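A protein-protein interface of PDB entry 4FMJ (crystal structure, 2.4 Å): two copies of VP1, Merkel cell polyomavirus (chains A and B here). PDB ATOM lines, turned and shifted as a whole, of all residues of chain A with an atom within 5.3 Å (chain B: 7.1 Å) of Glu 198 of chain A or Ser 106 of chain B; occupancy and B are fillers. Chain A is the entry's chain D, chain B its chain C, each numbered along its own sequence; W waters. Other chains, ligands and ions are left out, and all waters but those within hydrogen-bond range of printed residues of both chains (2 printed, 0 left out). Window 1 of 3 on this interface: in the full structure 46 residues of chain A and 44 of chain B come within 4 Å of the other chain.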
ATOM      1  N   ASN A  66      17.722 -12.416  -0.783  1.00  0.00           N
ATOM      2  CA  ASN A  66      18.492 -11.962   0.371  1.00  0.00           C
ATOM      3  C   ASN A  66      17.851 -10.786   1.119  1.00  0.00           C
ATOM      4  O   ASN A  66      18.528 -10.069   1.863  1.00  0.00           O
ATOM      5  CB  ASN A  66      19.927 -11.609  -0.031  1.00  0.00           C
ATOM      6  CG  ASN A  66      20.788 -12.835  -0.305  1.00  0.00           C
ATOM      7  OD1 ASN A  66      20.474 -13.964   0.100  1.00  0.00           O
ATOM      8  ND2 ASN A  66      21.888 -12.611  -1.001  1.00  0.00           N
ATOM      9  N   LEU A  67      16.550 -10.588   0.926  1.00  0.00           N
ATOM     10  CA  LEU A  67      15.852  -9.486   1.582  1.00  0.00           C
ATOM     11  C   LEU A  67      14.580  -9.966   2.279  1.00  0.00           C
ATOM     12  O   LEU A  67      13.506  -9.972   1.674  1.00  0.00           O
ATOM     13  CB  LEU A  67      15.537  -8.353   0.597  1.00  0.00           C
ATOM     14  CG  LEU A  67      16.686  -7.781  -0.236  1.00  0.00           C
ATOM     15  CD1 LEU A  67      16.136  -7.171  -1.515  1.00  0.00           C
ATOM     16  CD2 LEU A  67      17.551  -6.783   0.551  1.00  0.00           C
ATOM     17  N   PRO A  68      14.705 -10.373   3.562  1.00  0.00           N
ATOM     18  CA  PRO A  68      13.546 -10.737   4.376  1.00  0.00           C
ATOM     19  C   PRO A  68      12.555  -9.572   4.475  1.00  0.00           C
ATOM     20  O   PRO A  68      12.958  -8.418   4.664  1.00  0.00           O
ATOM     21  CB  PRO A  68      14.159 -11.040   5.748  1.00  0.00           C
ATOM     22  CG  PRO A  68      15.593 -11.370   5.463  1.00  0.00           C
ATOM     23  CD  PRO A  68      15.968 -10.502   4.313  1.00  0.00           C
ATOM     24  N   LEU A 147      14.450   3.957   5.783  1.00  0.00           N
ATOM     25  CA  LEU A 147      15.813   4.332   6.180  1.00  0.00           C
ATOM     26  C   LEU A 147      16.748   3.145   5.902  1.00  0.00           C
ATOM     27  O   LEU A 147      16.414   2.000   6.224  1.00  0.00           O
ATOM     28  CB  LEU A 147      15.871   4.753   7.660  1.00  0.00           C
ATOM     29  CG  LEU A 147      17.160   5.408   8.179  1.00  0.00           C
ATOM     30  CD1 LEU A 147      16.886   6.344   9.346  1.00  0.00           C
ATOM     31  CD2 LEU A 147      18.248   4.378   8.542  1.00  0.00           C
ATOM     32  N   VAL A 148      17.912   3.422   5.313  1.00  0.00           N
ATOM     33  CA  VAL A 148      18.857   2.362   4.918  1.00  0.00           C
ATOM     34  C   VAL A 148      20.266   2.575   5.459  1.00  0.00           C
ATOM     35  O   VAL A 148      20.669   3.706   5.748  1.00  0.00           O
ATOM     36  CB  VAL A 148      18.945   2.186   3.369  1.00  0.00           C
ATOM     37  CG1 VAL A 148      17.637   1.626   2.800  1.00  0.00           C
ATOM     38  CG2 VAL A 148      19.371   3.495   2.678  1.00  0.00           C
ATOM     39  N   LEU A 149      21.013   1.479   5.573  1.00  0.00           N
ATOM     40  CA  LEU A 149      22.419   1.532   5.991  1.00  0.00           C
ATOM     41  C   LEU A 149      23.276   2.346   5.017  1.00  0.00           C
ATOM     42  O   LEU A 149      24.127   3.145   5.438  1.00  0.00           O
ATOM     43  CB  LEU A 149      22.991   0.122   6.156  1.00  0.00           C
ATOM     44  CG  LEU A 149      24.322   0.035   6.914  1.00  0.00           C
ATOM     45  CD1 LEU A 149      24.141   0.322   8.398  1.00  0.00           C
ATOM     46  CD2 LEU A 149      24.966  -1.314   6.724  1.00  0.00           C
ATOM     47  N   TYR A 155      18.764  -1.703  -5.083  1.00  0.00           N
ATOM     48  CA  TYR A 155      17.734  -2.677  -4.799  1.00  0.00           C
ATOM     49  C   TYR A 155      17.076  -3.154  -6.094  1.00  0.00           C
ATOM     50  O   TYR A 155      17.062  -2.416  -7.072  1.00  0.00           O
ATOM     51  CB  TYR A 155      16.723  -2.084  -3.817  1.00  0.00           C
ATOM     52  CG  TYR A 155      17.271  -2.002  -2.408  1.00  0.00           C
ATOM     53  CD1 TYR A 155      17.304  -3.136  -1.582  1.00  0.00           C
ATOM     54  CD2 TYR A 155      17.779  -0.804  -1.904  1.00  0.00           C
ATOM     55  CE1 TYR A 155      17.820  -3.070  -0.295  1.00  0.00           C
ATOM     56  CE2 TYR A 155      18.300  -0.727  -0.619  1.00  0.00           C
ATOM     57  CZ  TYR A 155      18.313  -1.862   0.183  1.00  0.00           C
ATOM     58  OH  TYR A 155      18.824  -1.789   1.464  1.00  0.00           O
ATOM     59  N   PRO A 196      10.844  -4.944   2.282  1.00  0.00           N
ATOM     60  CA  PRO A 196      12.077  -5.355   2.953  1.00  0.00           C
ATOM     61  C   PRO A 196      12.268  -4.752   4.347  1.00  0.00           C
ATOM     62  O   PRO A 196      12.223  -3.529   4.526  1.00  0.00           O
ATOM     63  CB  PRO A 196      13.167  -4.867   1.996  1.00  0.00           C
ATOM     64  CG  PRO A 196      12.520  -4.927   0.661  1.00  0.00           C
ATOM     65  CD  PRO A 196      11.118  -4.440   0.922  1.00  0.00           C
ATOM     66  N   ILE A 197      12.491  -5.628   5.320  1.00  0.00           N
ATOM     67  CA  ILE A 197      12.719  -5.234   6.705  1.00  0.00           C
ATOM     68  C   ILE A 197      13.846  -4.200   6.817  1.00  0.00           C
ATOM     69  O   ILE A 197      13.740  -3.251   7.583  1.00  0.00           O
ATOM     70  CB  ILE A 197      12.985  -6.481   7.583  1.00  0.00           C
ATOM     71  CG1 ILE A 197      11.695  -7.291   7.723  1.00  0.00           C
ATOM     72  CG2 ILE A 197      13.528  -6.111   8.960  1.00  0.00           C
ATOM     73  CD1 ILE A 197      11.889  -8.767   7.982  1.00  0.00           C
ATOM     74  N   GLU A 198      14.900  -4.369   6.025  1.00  0.00           N
ATOM     75  CA  GLU A 198      16.085  -3.532   6.135  1.00  0.00           C
ATOM     76  C   GLU A 198      15.944  -2.138   5.497  1.00  0.00           C
ATOM     77  O   GLU A 198      16.839  -1.299   5.635  1.00  0.00           O
ATOM     78  CB  GLU A 198      17.313  -4.266   5.579  1.00  0.00           C
ATOM     79  CG  GLU A 198      17.341  -4.468   4.061  1.00  0.00           C
ATOM     80  CD  GLU A 198      18.691  -4.983   3.570  1.00  0.00           C
ATOM     81  OE1 GLU A 198      19.062  -6.131   3.927  1.00  0.00           O
ATOM     82  OE2 GLU A 198      19.374  -4.230   2.834  1.00  0.00           O
ATOM     83  N   VAL A 199      14.834  -1.919   4.794  1.00  0.00           N
ATOM     84  CA  VAL A 199      14.504  -0.617   4.220  1.00  0.00           C
ATOM     85  C   VAL A 199      13.434   0.098   5.062  1.00  0.00           C
ATOM     86  O   VAL A 199      13.479   1.319   5.216  1.00  0.00           O
ATOM     87  CB  VAL A 199      14.007  -0.744   2.733  1.00  0.00           C
ATOM     88  CG1 VAL A 199      13.705   0.616   2.133  1.00  0.00           C
ATOM     89  CG2 VAL A 199      15.027  -1.495   1.858  1.00  0.00           C
ATOM     90  N   TRP A 200      12.486  -0.671   5.611  1.00  0.00           N
ATOM     91  CA  TRP A 200      11.280  -0.109   6.240  1.00  0.00           C
ATOM     92  C   TRP A 200      11.110  -0.416   7.743  1.00  0.00           C
ATOM     93  O   TRP A 200      11.129  -1.581   8.154  1.00  0.00           O
ATOM     94  CB  TRP A 200      10.021  -0.585   5.491  1.00  0.00           C
ATOM     95  CG  TRP A 200       9.993  -0.267   4.021  1.00  0.00           C
ATOM     96  CD1 TRP A 200      10.126  -1.155   2.986  1.00  0.00           C
ATOM     97  CD2 TRP A 200       9.813   1.022   3.422  1.00  0.00           C
ATOM     98  NE1 TRP A 200      10.049  -0.495   1.782  1.00  0.00           N
ATOM     99  CE2 TRP A 200       9.857   0.842   2.021  1.00  0.00           C
ATOM    100  CE3 TRP A 200       9.627   2.318   3.933  1.00  0.00           C
ATOM    101  CZ2 TRP A 200       9.719   1.906   1.126  1.00  0.00           C
ATOM    102  CZ3 TRP A 200       9.484   3.381   3.038  1.00  0.00           C
ATOM    103  CH2 TRP A 200       9.532   3.166   1.650  1.00  0.00           C
ATOM    104  N   VAL B 102      14.609   5.693  15.439  1.00  0.00           N
ATOM    105  CA  VAL B 102      14.066   5.408  14.113  1.00  0.00           C
ATOM    106  C   VAL B 102      15.095   4.677  13.263  1.00  0.00           C
ATOM    107  O   VAL B 102      16.281   5.006  13.300  1.00  0.00           O
ATOM    108  CB  VAL B 102      13.621   6.716  13.410  1.00  0.00           C
ATOM    109  CG1 VAL B 102      12.932   6.426  12.086  1.00  0.00           C
ATOM    110  CG2 VAL B 102      12.682   7.514  14.320  1.00  0.00           C
ATOM    111  N   GLY B 103      14.638   3.673  12.517  1.00  0.00           N
ATOM    112  CA  GLY B 103      15.500   2.939  11.588  1.00  0.00           C
ATOM    113  C   GLY B 103      16.303   1.807  12.205  1.00  0.00           C
ATOM    114  O   GLY B 103      17.381   1.456  11.702  1.00  0.00           O
ATOM    115  N   ILE B 104      15.772   1.230  13.283  1.00  0.00           N
ATOM    116  CA  ILE B 104      16.407   0.114  13.975  1.00  0.00           C
ATOM    117  C   ILE B 104      16.518  -1.079  13.032  1.00  0.00           C
ATOM    118  O   ILE B 104      17.560  -1.739  12.966  1.00  0.00           O
ATOM    119  CB  ILE B 104      15.641  -0.257  15.272  1.00  0.00           C
ATOM    120  CG1 ILE B 104      15.954   0.759  16.366  1.00  0.00           C
ATOM    121  CG2 ILE B 104      15.998  -1.658  15.756  1.00  0.00           C
ATOM    122  CD1 ILE B 104      14.806   1.005  17.337  1.00  0.00           C
ATOM    123  N   SER B 105      15.459  -1.315  12.267  1.00  0.00           N
ATOM    124  CA  SER B 105      15.403  -2.454  11.344  1.00  0.00           C
ATOM    125  C   SER B 105      16.500  -2.442  10.267  1.00  0.00           C
ATOM    126  O   SER B 105      16.865  -3.495   9.760  1.00  0.00           O
ATOM    127  CB  SER B 105      14.020  -2.551  10.698  1.00  0.00           C
ATOM    128  OG  SER B 105      13.816  -1.474   9.806  1.00  0.00           O
ATOM    129  N   SER B 106      17.024  -1.257   9.934  1.00  0.00           N
ATOM    130  CA  SER B 106      18.086  -1.128   8.943  1.00  0.00           C
ATOM    131  C   SER B 106      19.355  -1.896   9.324  1.00  0.00           C
ATOM    132  O   SER B 106      20.148  -2.259   8.459  1.00  0.00           O
ATOM    133  CB  SER B 106      18.416   0.350   8.676  1.00  0.00           C
ATOM    134  OG  SER B 106      19.150   0.936   9.735  1.00  0.00           O
ATOM    135  N   LEU B 107      19.530  -2.160  10.614  1.00  0.00           N
ATOM    136  CA  LEU B 107      20.728  -2.840  11.102  1.00  0.00           C
ATOM    137  C   LEU B 107      20.709  -4.376  10.923  1.00  0.00           C
ATOM    138  O   LEU B 107      21.636  -5.065  11.365  1.00  0.00           O
ATOM    139  CB  LEU B 107      21.009  -2.457  12.563  1.00  0.00           C
ATOM    140  CG  LEU B 107      20.956  -0.981  12.967  1.00  0.00           C
ATOM    141  CD1 LEU B 107      21.245  -0.838  14.452  1.00  0.00           C
ATOM    142  CD2 LEU B 107      21.889  -0.076  12.125  1.00  0.00           C
ATOM    143  N   ILE B 108      19.677  -4.922  10.285  1.00  0.00           N
ATOM    144  CA  ILE B 108      19.752  -6.336   9.907  1.00  0.00           C
ATOM    145  C   ILE B 108      20.628  -6.558   8.663  1.00  0.00           C
ATOM    146  O   ILE B 108      20.957  -7.707   8.335  1.00  0.00           O
ATOM    147  CB  ILE B 108      18.367  -7.006   9.698  1.00  0.00           C
ATOM    148  CG1 ILE B 108      17.668  -6.436   8.456  1.00  0.00           C
ATOM    149  CG2 ILE B 108      17.520  -6.928  10.977  1.00  0.00           C
ATOM    150  CD1 ILE B 108      16.762  -7.413   7.790  1.00  0.00           C
ATOM    151  N   ASN B 109      20.990  -5.459   7.987  1.00  0.00           N
ATOM    152  CA  ASN B 109      21.875  -5.479   6.816  1.00  0.00           C
ATOM    153  C   ASN B 109      23.255  -6.077   7.120  1.00  0.00           C
ATOM    154  O   ASN B 109      24.091  -5.434   7.762  1.00  0.00           O
ATOM    155  CB  ASN B 109      22.033  -4.049   6.258  1.00  0.00           C
ATOM    156  CG  ASN B 109      22.753  -3.992   4.899  1.00  0.00           C
ATOM    157  OD1 ASN B 109      23.443  -4.926   4.484  1.00  0.00           O
ATOM    158  ND2 ASN B 109      22.594  -2.871   4.211  1.00  0.00           N
ATOM    159  N   VAL B 110      23.478  -7.303   6.651  1.00  0.00           N
ATOM    160  CA  VAL B 110      24.758  -7.993   6.835  1.00  0.00           C
ATOM    161  C   VAL B 110      25.456  -8.282   5.497  1.00  0.00           C
ATOM    162  O   VAL B 110      26.325  -9.163   5.411  1.00  0.00           O
ATOM    163  CB  VAL B 110      24.594  -9.305   7.651  1.00  0.00           C
ATOM    164  CG1 VAL B 110      24.275  -8.997   9.119  1.00  0.00           C
ATOM    165  CG2 VAL B 110      23.527 -10.226   7.028  1.00  0.00           C
ATOM    166  N   HIS B 111      25.084  -7.535   4.457  1.00  0.00           N
ATOM    167  CA  HIS B 111      25.661  -7.721   3.124  1.00  0.00           C
ATOM    168  C   HIS B 111      26.222  -6.442   2.502  1.00  0.00           C
ATOM    169  O   HIS B 111      26.564  -6.439   1.325  1.00  0.00           O
ATOM    170  CB  HIS B 111      24.641  -8.364   2.170  1.00  0.00           C
ATOM    171  CG  HIS B 111      23.323  -7.656   2.139  1.00  0.00           C
ATOM    172  ND1 HIS B 111      23.179  -6.370   1.657  1.00  0.00           N
ATOM    173  CD2 HIS B 111      22.093  -8.044   2.552  1.00  0.00           C
ATOM    174  CE1 HIS B 111      21.915  -6.001   1.770  1.00  0.00           C
ATOM    175  NE2 HIS B 111      21.235  -6.998   2.311  1.00  0.00           N
ATOM    176  N   TYR B 112      26.315  -5.361   3.270  1.00  0.00           N
ATOM    177  CA  TYR B 112      26.969  -4.148   2.780  1.00  0.00           C
ATOM    178  C   TYR B 112      28.323  -4.519   2.171  1.00  0.00           C
ATOM    179  O   TYR B 112      29.090  -5.297   2.765  1.00  0.00           O
ATOM    180  CB  TYR B 112      27.134  -3.139   3.915  1.00  0.00           C
ATOM    181  CG  TYR B 112      28.041  -1.962   3.613  1.00  0.00           C
ATOM    182  CD1 TYR B 112      27.742  -1.059   2.587  1.00  0.00           C
ATOM    183  CD2 TYR B 112      29.189  -1.741   4.370  1.00  0.00           C
ATOM    184  CE1 TYR B 112      28.580   0.032   2.320  1.00  0.00           C
ATOM    185  CE2 TYR B 112      30.026  -0.662   4.118  1.00  0.00           C
ATOM    186  CZ  TYR B 112      29.722   0.223   3.093  1.00  0.00           C
ATOM    187  OH  TYR B 112      30.564   1.290   2.851  1.00  0.00           O
ATOM    188  N   VAL B 127      26.323  -4.156  12.691  1.00  0.00           N
ATOM    189  CA  VAL B 127      26.612  -2.971  13.495  1.00  0.00           C
ATOM    190  C   VAL B 127      26.414  -3.352  14.957  1.00  0.00           C
ATOM    191  O   VAL B 127      25.362  -3.849  15.344  1.00  0.00           O
ATOM    192  CB  VAL B 127      25.754  -1.753  13.073  1.00  0.00           C
ATOM    193  CG1 VAL B 127      26.086  -0.540  13.915  1.00  0.00           C
ATOM    194  CG2 VAL B 127      25.960  -1.441  11.573  1.00  0.00           C
ATOM    195  N   HIS B 272      28.369   4.682  14.172  1.00  0.00           N
ATOM    196  CA  HIS B 272      27.115   4.945  13.455  1.00  0.00           C
ATOM    197  C   HIS B 272      26.024   5.439  14.419  1.00  0.00           C
ATOM    198  O   HIS B 272      25.993   5.030  15.591  1.00  0.00           O
ATOM    199  CB  HIS B 272      26.695   3.661  12.730  1.00  0.00           C
ATOM    200  CG  HIS B 272      25.472   3.786  11.875  1.00  0.00           C
ATOM    201  ND1 HIS B 272      25.273   4.828  10.996  1.00  0.00           N
ATOM    202  CD2 HIS B 272      24.414   2.955  11.718  1.00  0.00           C
ATOM    203  CE1 HIS B 272      24.128   4.651  10.359  1.00  0.00           C
ATOM    204  NE2 HIS B 272      23.587   3.521  10.779  1.00  0.00           N
ATOM    205  N   LEU B 274      21.605   6.818  14.800  1.00  0.00           N
ATOM    206  CA  LEU B 274      20.239   6.749  14.270  1.00  0.00           C
ATOM    207  C   LEU B 274      19.398   7.940  14.741  1.00  0.00           C
ATOM    208  O   LEU B 274      19.708   8.547  15.769  1.00  0.00           O
ATOM    209  CB  LEU B 274      19.553   5.422  14.669  1.00  0.00           C
ATOM    210  CG  LEU B 274      19.965   4.108  13.985  1.00  0.00           C
ATOM    211  CD1 LEU B 274      19.116   2.937  14.486  1.00  0.00           C
ATOM    212  CD2 LEU B 274      19.898   4.181  12.466  1.00  0.00           C
HETATM  213  O   HOH W   1      19.777  -1.306   5.812  1.00  0.00           O
HETATM  214  O   HOH W   2      14.639   1.184   8.687  1.00  0.00           O
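Hydrophobic or aromatic side chains of chain A within 4 Å of the printed part of chain B: Leu 147, Leu 149 and Ile 197.
Among the printed residues, 11 pairs touch across the chains.
Among the printed residues, no Asp or Glu carboxylate lies within 4 Å of a Lys or Arg side-chain nitrogen of the other chain.
The side-chain amide oxygen (OD1) of Asn 109 of chain B sits at hydrogen-bond distance from the backbone NH (N) of Tyr 112 of chain B (3.1 Å).
N of Ile 197 of chain A lies within hydrogen-bond range of O of Pro 68 of chain A (2.9 Å).
The backbone NH of Leu 147 of chain A lies within hydrogen-bond range of the backbone carbonyl oxygen of Val 199 of chain A, 2.9 Å away.
The backbone NH (N) of His 111 of chain B is in hydrogen-bond range of the side-chain amide oxygen (OD1) of Asn 109 of chain B, 3.1 Å away.
The side-chain carboxylate (OE2) of Glu 198 of chain A lies within hydrogen-bond range of the side-chain hydroxyl (OH) of Tyr 155 of chain A (2.9 Å).
The side-chain hydroxyl (OG) of Ser 106 of chain B is in hydrogen-bond range of the backbone carbonyl oxygen (O) of Gly 103 of chain B (2.7 Å).
Ser 106 of chain B touches Leu 147 of chain A.
Leu 149 of chain A touches Asn 109 of chain B (CB to ND2, 3.6 Å).
Leu 149 of chain A touches Tyr 112 of chain B (CD2 to CB, 3.99 Å).
CG2 of Ile 197 of chain A touches CD1 of Ile 108 of chain B (3.7 Å).
Ser 105 of chain B touches Glu 198 of chain A.
O of Glu 198 of chain A touches CA of Ser 106 of chain B, 3.5 Å away.
Ile 108 of chain B touches Glu 198 of chain A (CG1 to CB, 3.6 Å).
OE2 of Glu 198 of chain A touches ND2 of Asn 109 of chain B, at 3.8 Å.
No position is printed for both chains.
Of the 11 pairs that touch across the chains among the printed residues, none has its exchanged pair printed and touching as well.
OG of Ser 105 of chain B sits at hydrogen-bond distance from O of Trp 200 of chain A.
OG of Ser 105 of chain B sits at hydrogen-bond distance from O of Ile 197 of chain A (2.8 Å).
A ring nitrogen (NE2) of His 111 of chain B is in hydrogen-bond range of the side-chain carboxylate of Glu 198 of chain A (2.8 Å).
Water W1 lies within hydrogen-bond range of the backbone carbonyl oxygen (O) of Ser 106 of chain B (2.8 Å), the backbone carbonyl oxygen (O) of Glu 198 of chain A (2.9 Å) and the backbone NH (N) of Leu 149 of chain A (3.1 Å).
Water W2 bridges the side-chain hydroxyl of Ser 105 of chain B (3.0 Å) and the backbone carbonyl oxygen of Leu 147 of chain A (3.1 Å).
Printed residues of chain B within 4 Å of Leu 147 of chain A: Ser 106.
Of the printed residues of chain B, Glu 198 of chain A touches Ser 105 (3.7 Å), Ser 106 (3.5 Å), Ile 108 (3.6 Å), Asn 109 (3.8 Å) and His 111 (2.8 Å).
Of the printed residues of chain B, Trp 200 of chain A touches Ser 105 (3.2 Å).
Gly 103 of chain B touches none of the printed residues of chain A.
Ser 106 of chain B touches just these residues of chain A: Leu 147 and Glu 198.
Of the printed residues of chain A, Asn 109 of chain B touches Leu 149 and Glu 198.
The nearest residue of chain A that does not touch Ser 106 of chain B is Leu 149 of chain A (4.2 Å).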
